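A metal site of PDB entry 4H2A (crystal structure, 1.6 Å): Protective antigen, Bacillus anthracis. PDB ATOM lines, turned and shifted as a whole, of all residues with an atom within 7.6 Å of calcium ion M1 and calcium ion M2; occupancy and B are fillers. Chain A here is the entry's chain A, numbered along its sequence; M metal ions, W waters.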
ATOM      1  N   PRO A 176      26.902 -15.773   9.986  1.00  0.00           N
ATOM      2  CA  PRO A 176      25.794 -15.137   9.304  1.00  0.00           C
ATOM      3  C   PRO A 176      24.584 -15.083  10.229  1.00  0.00           C
ATOM      4  O   PRO A 176      24.161 -16.095  10.738  1.00  0.00           O
ATOM      5  CB  PRO A 176      25.559 -16.039   8.099  1.00  0.00           C
ATOM      6  CG  PRO A 176      26.920 -16.652   7.852  1.00  0.00           C
ATOM      7  CD  PRO A 176      27.373 -16.946   9.239  1.00  0.00           C
ATOM      8  N   ASP A 177      24.112 -13.867  10.450  1.00  0.00           N
ATOM      9  CA  ASP A 177      23.001 -13.583  11.373  1.00  0.00           C
ATOM     10  C   ASP A 177      22.375 -12.274  10.877  1.00  0.00           C
ATOM     11  O   ASP A 177      22.530 -11.206  11.495  1.00  0.00           O
ATOM     12  CB  ASP A 177      23.511 -13.478  12.791  1.00  0.00           C
ATOM     13  CG  ASP A 177      22.406 -13.174  13.787  1.00  0.00           C
ATOM     14  OD1 ASP A 177      21.258 -13.486  13.447  1.00  0.00           O
ATOM     15  OD2 ASP A 177      22.689 -12.650  14.858  1.00  0.00           O
ATOM     16  N   ARG A 178      21.671 -12.377   9.761  1.00  0.00           N
ATOM     17  CA  ARG A 178      21.201 -11.196   9.015  1.00  0.00           C
ATOM     18  C   ARG A 178      20.323 -10.292   9.888  1.00  0.00           C
ATOM     19  O   ARG A 178      20.427  -9.068   9.843  1.00  0.00           O
ATOM     20  CB  ARG A 178      20.452 -11.573   7.712  1.00  0.00           C
ATOM     21  CG  ARG A 178      19.933 -10.395   6.902  1.00  0.00           C
ATOM     22  CD  ARG A 178      21.058  -9.516   6.360  1.00  0.00           C
ATOM     23  NE  ARG A 178      20.588  -8.414   5.502  1.00  0.00           N
ATOM     24  CZ  ARG A 178      20.161  -7.227   5.928  1.00  0.00           C
ATOM     25  NH1 ARG A 178      20.103  -6.941   7.222  1.00  0.00           N
ATOM     26  NH2 ARG A 178      19.762  -6.309   5.049  1.00  0.00           N
ATOM     27  N   ASP A 179      19.473 -10.891  10.705  1.00  0.00           N
ATOM     28  CA  ASP A 179      18.571 -10.090  11.506  1.00  0.00           C
ATOM     29  C   ASP A 179      19.090  -9.704  12.889  1.00  0.00           C
ATOM     30  O   ASP A 179      18.398  -9.020  13.649  1.00  0.00           O
ATOM     31  CB  ASP A 179      17.214 -10.787  11.628  1.00  0.00           C
ATOM     32  CG  ASP A 179      17.313 -12.174  12.254  1.00  0.00           C
ATOM     33  OD1 ASP A 179      18.372 -12.523  12.820  1.00  0.00           O
ATOM     34  OD2 ASP A 179      16.328 -12.899  12.120  1.00  0.00           O
ATOM     35  N   ASN A 180      20.327 -10.096  13.230  1.00  0.00           N
ATOM     36  CA  ASN A 180      20.964  -9.715  14.499  1.00  0.00           C
ATOM     37  C   ASN A 180      20.210 -10.169  15.764  1.00  0.00           C
ATOM     38  O   ASN A 180      20.357  -9.554  16.813  1.00  0.00           O
ATOM     39  CB  ASN A 180      21.220  -8.180  14.519  1.00  0.00           C
ATOM     40  CG  ASN A 180      22.405  -7.784  15.399  1.00  0.00           C
ATOM     41  OD1 ASN A 180      23.497  -8.353  15.251  1.00  0.00           O
ATOM     42  ND2 ASN A 180      22.196  -6.852  16.315  1.00  0.00           N
ATOM     43  N   ASP A 181      19.458 -11.272  15.697  1.00  0.00           N
ATOM     44  CA  ASP A 181      18.847 -11.819  16.911  1.00  0.00           C
ATOM     45  C   ASP A 181      19.791 -12.715  17.669  1.00  0.00           C
ATOM     46  O   ASP A 181      19.553 -13.010  18.819  1.00  0.00           O
ATOM     47  CB  ASP A 181      17.463 -12.481  16.677  1.00  0.00           C
ATOM     48  CG  ASP A 181      17.460 -13.632  15.707  1.00  0.00           C
ATOM     49  OD1 ASP A 181      18.533 -14.248  15.411  1.00  0.00           O
ATOM     50  OD2 ASP A 181      16.357 -13.965  15.195  1.00  0.00           O
ATOM     51  N   GLY A 182      20.889 -13.121  17.037  1.00  0.00           N
ATOM     52  CA  GLY A 182      21.849 -13.989  17.722  1.00  0.00           C
ATOM     53  C   GLY A 182      21.840 -15.417  17.235  1.00  0.00           C
ATOM     54  O   GLY A 182      22.776 -16.191  17.519  1.00  0.00           O
ATOM     55  N   ILE A 183      20.763 -15.811  16.553  1.00  0.00           N
ATOM     56  CA  ILE A 183      20.634 -17.201  16.082  1.00  0.00           C
ATOM     57  C   ILE A 183      21.160 -17.242  14.650  1.00  0.00           C
ATOM     58  O   ILE A 183      20.658 -16.550  13.764  1.00  0.00           O
ATOM     59  CB  ILE A 183      19.174 -17.751  16.105  1.00  0.00           C
ATOM     60  CG1 ILE A 183      18.449 -17.456  17.416  1.00  0.00           C
ATOM     61  CG2 ILE A 183      19.161 -19.268  15.829  1.00  0.00           C
ATOM     62  CD1 ILE A 183      16.993 -17.916  17.437  1.00  0.00           C
ATOM     63  N   PRO A 184      22.193 -18.058  14.391  1.00  0.00           N
ATOM     64  CA  PRO A 184      22.706 -18.104  13.028  1.00  0.00           C
ATOM     65  C   PRO A 184      21.647 -18.408  11.969  1.00  0.00           C
ATOM     66  O   PRO A 184      20.759 -19.249  12.206  1.00  0.00           O
ATOM     67  CB  PRO A 184      23.741 -19.240  13.090  1.00  0.00           C
ATOM     68  CG  PRO A 184      24.190 -19.283  14.484  1.00  0.00           C
ATOM     69  CD  PRO A 184      22.940 -18.951  15.309  1.00  0.00           C
ATOM     70  N   ASP A 185      21.775 -17.781  10.794  1.00  0.00           N
ATOM     71  CA  ASP A 185      20.896 -17.994   9.627  1.00  0.00           C
ATOM     72  C   ASP A 185      20.560 -19.470   9.428  1.00  0.00           C
ATOM     73  O   ASP A 185      19.387 -19.854   9.349  1.00  0.00           O
ATOM     74  CB  ASP A 185      21.533 -17.518   8.315  1.00  0.00           C
ATOM     75  CG  ASP A 185      21.694 -16.004   8.211  1.00  0.00           C
ATOM     76  OD1 ASP A 185      21.318 -15.248   9.124  1.00  0.00           O
ATOM     77  OD2 ASP A 185      22.245 -15.590   7.178  1.00  0.00           O
ATOM     78  N   SER A 186      21.602 -20.312   9.345  1.00  0.00           N
ATOM     79  CA  SER A 186      21.430 -21.726   9.043  1.00  0.00           C
ATOM     80  C   SER A 186      20.557 -22.463  10.041  1.00  0.00           C
ATOM     81  O   SER A 186      19.731 -23.294   9.657  1.00  0.00           O
ATOM     82  CB  SER A 186      22.805 -22.420   8.924  1.00  0.00           C
ATOM     83  OG  SER A 186      23.505 -22.482  10.168  1.00  0.00           O
ATOM     84  N   GLU A 188      18.238 -21.145  12.036  1.00  0.00           N
ATOM     85  CA  GLU A 188      16.828 -20.690  11.955  1.00  0.00           C
ATOM     86  C   GLU A 188      16.075 -21.403  10.848  1.00  0.00           C
ATOM     87  O   GLU A 188      14.932 -21.800  11.019  1.00  0.00           O
ATOM     88  CB  GLU A 188      16.727 -19.162  11.783  1.00  0.00           C
ATOM     89  CG  GLU A 188      17.263 -18.371  12.949  1.00  0.00           C
ATOM     90  CD  GLU A 188      16.684 -16.975  13.040  1.00  0.00           C
ATOM     91  OE1 GLU A 188      17.372 -15.970  12.825  1.00  0.00           O
ATOM     92  OE2 GLU A 188      15.482 -16.874  13.345  1.00  0.00           O
ATOM     93  N   TYR A 192      16.260 -25.822  15.080  1.00  0.00           N
ATOM     94  CA  TYR A 192      17.082 -25.823  16.285  1.00  0.00           C
ATOM     95  C   TYR A 192      16.243 -26.162  17.487  1.00  0.00           C
ATOM     96  O   TYR A 192      15.005 -26.196  17.406  1.00  0.00           O
ATOM     97  CB  TYR A 192      17.757 -24.440  16.474  1.00  0.00           C
ATOM     98  CG  TYR A 192      16.795 -23.229  16.543  1.00  0.00           C
ATOM     99  CD1 TYR A 192      16.429 -22.655  17.762  1.00  0.00           C
ATOM    100  CD2 TYR A 192      16.287 -22.662  15.377  1.00  0.00           C
ATOM    101  CE1 TYR A 192      15.553 -21.563  17.827  1.00  0.00           C
ATOM    102  CE2 TYR A 192      15.450 -21.546  15.420  1.00  0.00           C
ATOM    103  CZ  TYR A 192      15.094 -21.000  16.643  1.00  0.00           C
ATOM    104  OH  TYR A 192      14.231 -19.915  16.644  1.00  0.00           O
ATOM    105  N   SER A 221      12.513 -20.612  12.419  1.00  0.00           N
ATOM    106  CA  SER A 221      12.209 -19.174  12.460  1.00  0.00           C
ATOM    107  C   SER A 221      12.814 -18.462  11.242  1.00  0.00           C
ATOM    108  O   SER A 221      13.603 -19.079  10.489  1.00  0.00           O
ATOM    109  CB  SER A 221      12.654 -18.568  13.796  1.00  0.00           C
ATOM    110  OG  SER A 221      13.998 -18.858  14.133  1.00  0.00           O
ATOM    111  N   SER A 222      12.395 -17.237  10.965  1.00  0.00           N
ATOM    112  CA  SER A 222      12.971 -16.495   9.835  1.00  0.00           C
ATOM    113  C   SER A 222      14.330 -15.888  10.170  1.00  0.00           C
ATOM    114  O   SER A 222      14.471 -15.167  11.181  1.00  0.00           O
ATOM    115  CB  SER A 222      12.064 -15.366   9.403  1.00  0.00           C
ATOM    116  OG  SER A 222      12.730 -14.584   8.452  1.00  0.00           O
ATOM    117  N   PRO A 223      15.343 -16.155   9.330  1.00  0.00           N
ATOM    118  CA  PRO A 223      16.631 -15.512   9.507  1.00  0.00           C
ATOM    119  C   PRO A 223      16.658 -14.052   9.084  1.00  0.00           C
ATOM    120  O   PRO A 223      17.663 -13.352   9.269  1.00  0.00           O
ATOM    121  CB  PRO A 223      17.556 -16.368   8.633  1.00  0.00           C
ATOM    122  CG  PRO A 223      16.676 -16.757   7.481  1.00  0.00           C
ATOM    123  CD  PRO A 223      15.328 -17.024   8.141  1.00  0.00           C
ATOM    124  N   GLU A 224      15.566 -13.562   8.516  1.00  0.00           N
ATOM    125  CA  GLU A 224      15.431 -12.167   8.166  1.00  0.00           C
ATOM    126  C   GLU A 224      14.492 -11.353   9.049  1.00  0.00           C
ATOM    127  O   GLU A 224      14.413 -10.132   8.877  1.00  0.00           O
ATOM    128  CB  GLU A 224      15.002 -12.055   6.709  1.00  0.00           C
ATOM    129  CG  GLU A 224      15.963 -12.815   5.805  1.00  0.00           C
ATOM    130  CD  GLU A 224      16.188 -12.206   4.443  1.00  0.00           C
ATOM    131  OE1 GLU A 224      16.065 -10.966   4.308  1.00  0.00           O
ATOM    132  OE2 GLU A 224      16.505 -12.974   3.505  1.00  0.00           O
ATOM    133  N   LYS A 225      13.864 -12.001  10.030  1.00  0.00           N
ATOM    134  CA  LYS A 225      13.002 -11.302  10.983  1.00  0.00           C
ATOM    135  C   LYS A 225      13.539 -11.534  12.381  1.00  0.00           C
ATOM    136  O   LYS A 225      13.602 -12.659  12.882  1.00  0.00           O
ATOM    137  CB  LYS A 225      11.545 -11.813  10.881  1.00  0.00           C
ATOM    138  CG  LYS A 225      10.854 -11.540   9.535  1.00  0.00           C
ATOM    139  CD  LYS A 225       9.420 -12.080   9.456  1.00  0.00           C
ATOM    140  CE  LYS A 225       8.402 -11.395  10.389  1.00  0.00           C
ATOM    141  NZ  LYS A 225       8.076  -9.998  10.052  1.00  0.00           N
ATOM    142  N   TRP A 226      13.971 -10.439  12.992  1.00  0.00           N
ATOM    143  CA  TRP A 226      14.417 -10.428  14.367  1.00  0.00           C
ATOM    144  C   TRP A 226      13.397 -11.046  15.302  1.00  0.00           C
ATOM    145  O   TRP A 226      13.752 -11.843  16.188  1.00  0.00           O
ATOM    146  CB  TRP A 226      14.771  -8.987  14.719  1.00  0.00           C
ATOM    147  CG  TRP A 226      15.243  -8.743  16.112  1.00  0.00           C
ATOM    148  CD1 TRP A 226      16.537  -8.803  16.588  1.00  0.00           C
ATOM    149  CD2 TRP A 226      14.434  -8.303  17.231  1.00  0.00           C
ATOM    150  NE1 TRP A 226      16.582  -8.494  17.913  1.00  0.00           N
ATOM    151  CE2 TRP A 226      15.347  -8.175  18.367  1.00  0.00           C
ATOM    152  CE3 TRP A 226      13.066  -8.070  17.427  1.00  0.00           C
ATOM    153  CZ2 TRP A 226      14.902  -7.781  19.618  1.00  0.00           C
ATOM    154  CZ3 TRP A 226      12.634  -7.664  18.691  1.00  0.00           C
ATOM    155  CH2 TRP A 226      13.536  -7.544  19.763  1.00  0.00           C
ATOM    156  N   SER A 227      12.125 -10.674  15.142  1.00  0.00           N
ATOM    157  CA  SER A 227      10.979 -11.398  15.696  1.00  0.00           C
ATOM    158  C   SER A 227      10.132 -11.984  14.578  1.00  0.00           C
ATOM    159  O   SER A 227       9.497 -11.240  13.752  1.00  0.00           O
ATOM    160  CB  SER A 227      10.090 -10.471  16.512  1.00  0.00           C
ATOM    161  OG  SER A 227       8.944 -11.159  16.918  1.00  0.00           O
ATOM    162  N   THR A 228      10.106 -13.307  14.465  1.00  0.00           N
ATOM    163  CA  THR A 228       9.411 -13.938  13.345  1.00  0.00           C
ATOM    164  C   THR A 228       7.900 -13.722  13.367  1.00  0.00           C
ATOM    165  O   THR A 228       7.280 -13.635  12.326  1.00  0.00           O
ATOM    166  CB  THR A 228       9.807 -15.424  13.220  1.00  0.00           C
ATOM    167  OG1 THR A 228      11.190 -15.478  12.872  1.00  0.00           O
ATOM    168  CG2 THR A 228       8.996 -16.109  12.111  1.00  0.00           C
ATOM    169  N   SER A 234      12.658 -10.856  20.495  1.00  0.00           N
ATOM    170  CA  SER A 234      13.380 -11.550  19.435  1.00  0.00           C
ATOM    171  C   SER A 234      13.224 -13.088  19.535  1.00  0.00           C
ATOM    172  O   SER A 234      12.848 -13.640  20.538  1.00  0.00           O
ATOM    173  CB  SER A 234      14.872 -11.215  19.397  1.00  0.00           C
ATOM    174  OG  SER A 234      15.607 -12.129  20.218  1.00  0.00           O
ATOM    175  N   ASP A 235      13.496 -13.738  18.433  1.00  0.00           N
ATOM    176  CA  ASP A 235      13.419 -15.199  18.361  1.00  0.00           C
ATOM    177  C   ASP A 235      14.373 -15.809  19.426  1.00  0.00           C
ATOM    178  O   ASP A 235      14.045 -16.814  20.027  1.00  0.00           O
ATOM    179  CB  ASP A 235      13.812 -15.612  16.959  1.00  0.00           C
ATOM    180  CG  ASP A 235      12.821 -15.175  15.878  1.00  0.00           C
ATOM    181  OD1 ASP A 235      11.634 -14.932  16.180  1.00  0.00           O
ATOM    182  OD2 ASP A 235      13.243 -15.107  14.718  1.00  0.00           O
ATOM    183  N   PHE A 236      15.532 -15.182  19.620  1.00  0.00           N
ATOM    184  CA  PHE A 236      16.561 -15.622  20.583  1.00  0.00           C
ATOM    185  C   PHE A 236      16.148 -15.314  21.987  1.00  0.00           C
ATOM    186  O   PHE A 236      16.312 -16.117  22.907  1.00  0.00           O
ATOM    187  CB  PHE A 236      17.892 -14.959  20.247  1.00  0.00           C
ATOM    188  CG  PHE A 236      19.034 -15.336  21.140  1.00  0.00           C
ATOM    189  CD1 PHE A 236      19.667 -16.565  21.023  1.00  0.00           C
ATOM    190  CD2 PHE A 236      19.532 -14.404  22.059  1.00  0.00           C
ATOM    191  CE1 PHE A 236      20.731 -16.890  21.863  1.00  0.00           C
ATOM    192  CE2 PHE A 236      20.599 -14.726  22.886  1.00  0.00           C
ATOM    193  CZ  PHE A 236      21.199 -15.960  22.760  1.00  0.00           C
ATOM    194  N   PRO A 254       8.998 -18.893  18.737  1.00  0.00           N
ATOM    195  CA  PRO A 254       9.163 -17.826  17.775  1.00  0.00           C
ATOM    196  C   PRO A 254       8.034 -17.647  16.769  1.00  0.00           C
ATOM    197  O   PRO A 254       7.975 -16.597  16.142  1.00  0.00           O
ATOM    198  CB  PRO A 254      10.492 -18.192  17.051  1.00  0.00           C
ATOM    199  CG  PRO A 254      11.221 -18.963  18.079  1.00  0.00           C
ATOM    200  CD  PRO A 254      10.185 -19.770  18.808  1.00  0.00           C
HETATM  201 CA    CA M   1      19.295 -14.694  13.201  1.00  0.00          CA
HETATM  202 CA    CA M   2      15.025 -14.526  13.324  1.00  0.00          CA
HETATM  203  O   HOH W   1      19.571 -14.758  10.871  1.00  0.00           O
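O of Ser 222 is bound to calcium ion M2 (2.3 Å). OD2 of Asp 235 is bound to calcium ion M2, at 2.3 Å. Calcium ion M2 is bound by OD2 of Asp 181. O of Lys 225 binds calcium ion M2 (2.4 Å). Calcium ion M2 is bound by OE2 of Glu 188 (2.4 Å). Calcium ion M2 is bound by OD2 of Asp 179. The side-chain carboxylate (OE1) of Glu 188 binds calcium ion M2 (2.8 Å). Calcium ion M2 has seven donor atoms within binding distance.
Calcium ion M1 is bound by OD1 of Asp 177 (2.3 Å), OE1 of Glu 188 (2.3 Å), water W1 (2.3 Å), O of Ile 183 (2.4 Å), OD1 of Asp 181 (2.4 Å) and OD1 of Asp 179 (2.4 Å).
Five residues have an atom within 4 Å of calcium ion M1: Asp 177, Asp 179, Asp 181, Ile 183 and Glu 188.
Water W1 lies within hydrogen-bond range of OD1 of Asp 185, O of Pro 223 and N of Arg 178.
Residues that only touch calcium ion M2: Thr 228 (3.98 Å). Seven residues have an atom within 4 Å of calcium ion M2: Asp 179, Asp 181, Glu 188, Ser 222, Lys 225, Thr 228 and Asp 235. Along chain A the residues within 4 Å of calcium ion M2 span positions 179 to 235.
The backbone NH (N) of Lys 225 lies within hydrogen-bond range of the side-chain hydroxyl (OG) of Ser 222, at 3.2 Å. The backbone NH of Ser 222 lies within hydrogen-bond range of the side-chain hydroxyl of Thr 228, at 2.9 Å. OG of Ser 222 sits at hydrogen-bond distance from N of Glu 224 (3.0 Å). N of Gly 182 sits at hydrogen-bond distance from OD2 of Asp 177, 2.9 Å away. The backbone NH (N) of Asp 177 lies close to the side-chain carboxylate (OD1) of Asp 185. N of Asp 235 lies within hydrogen-bond range of O of Trp 226. O of Glu 188 lies within hydrogen-bond range of N of Ser 221 (3.0 Å). The backbone NH (N) of Asp 179 lies close to the backbone carbonyl oxygen (O) of Pro 223 (3.4 Å).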
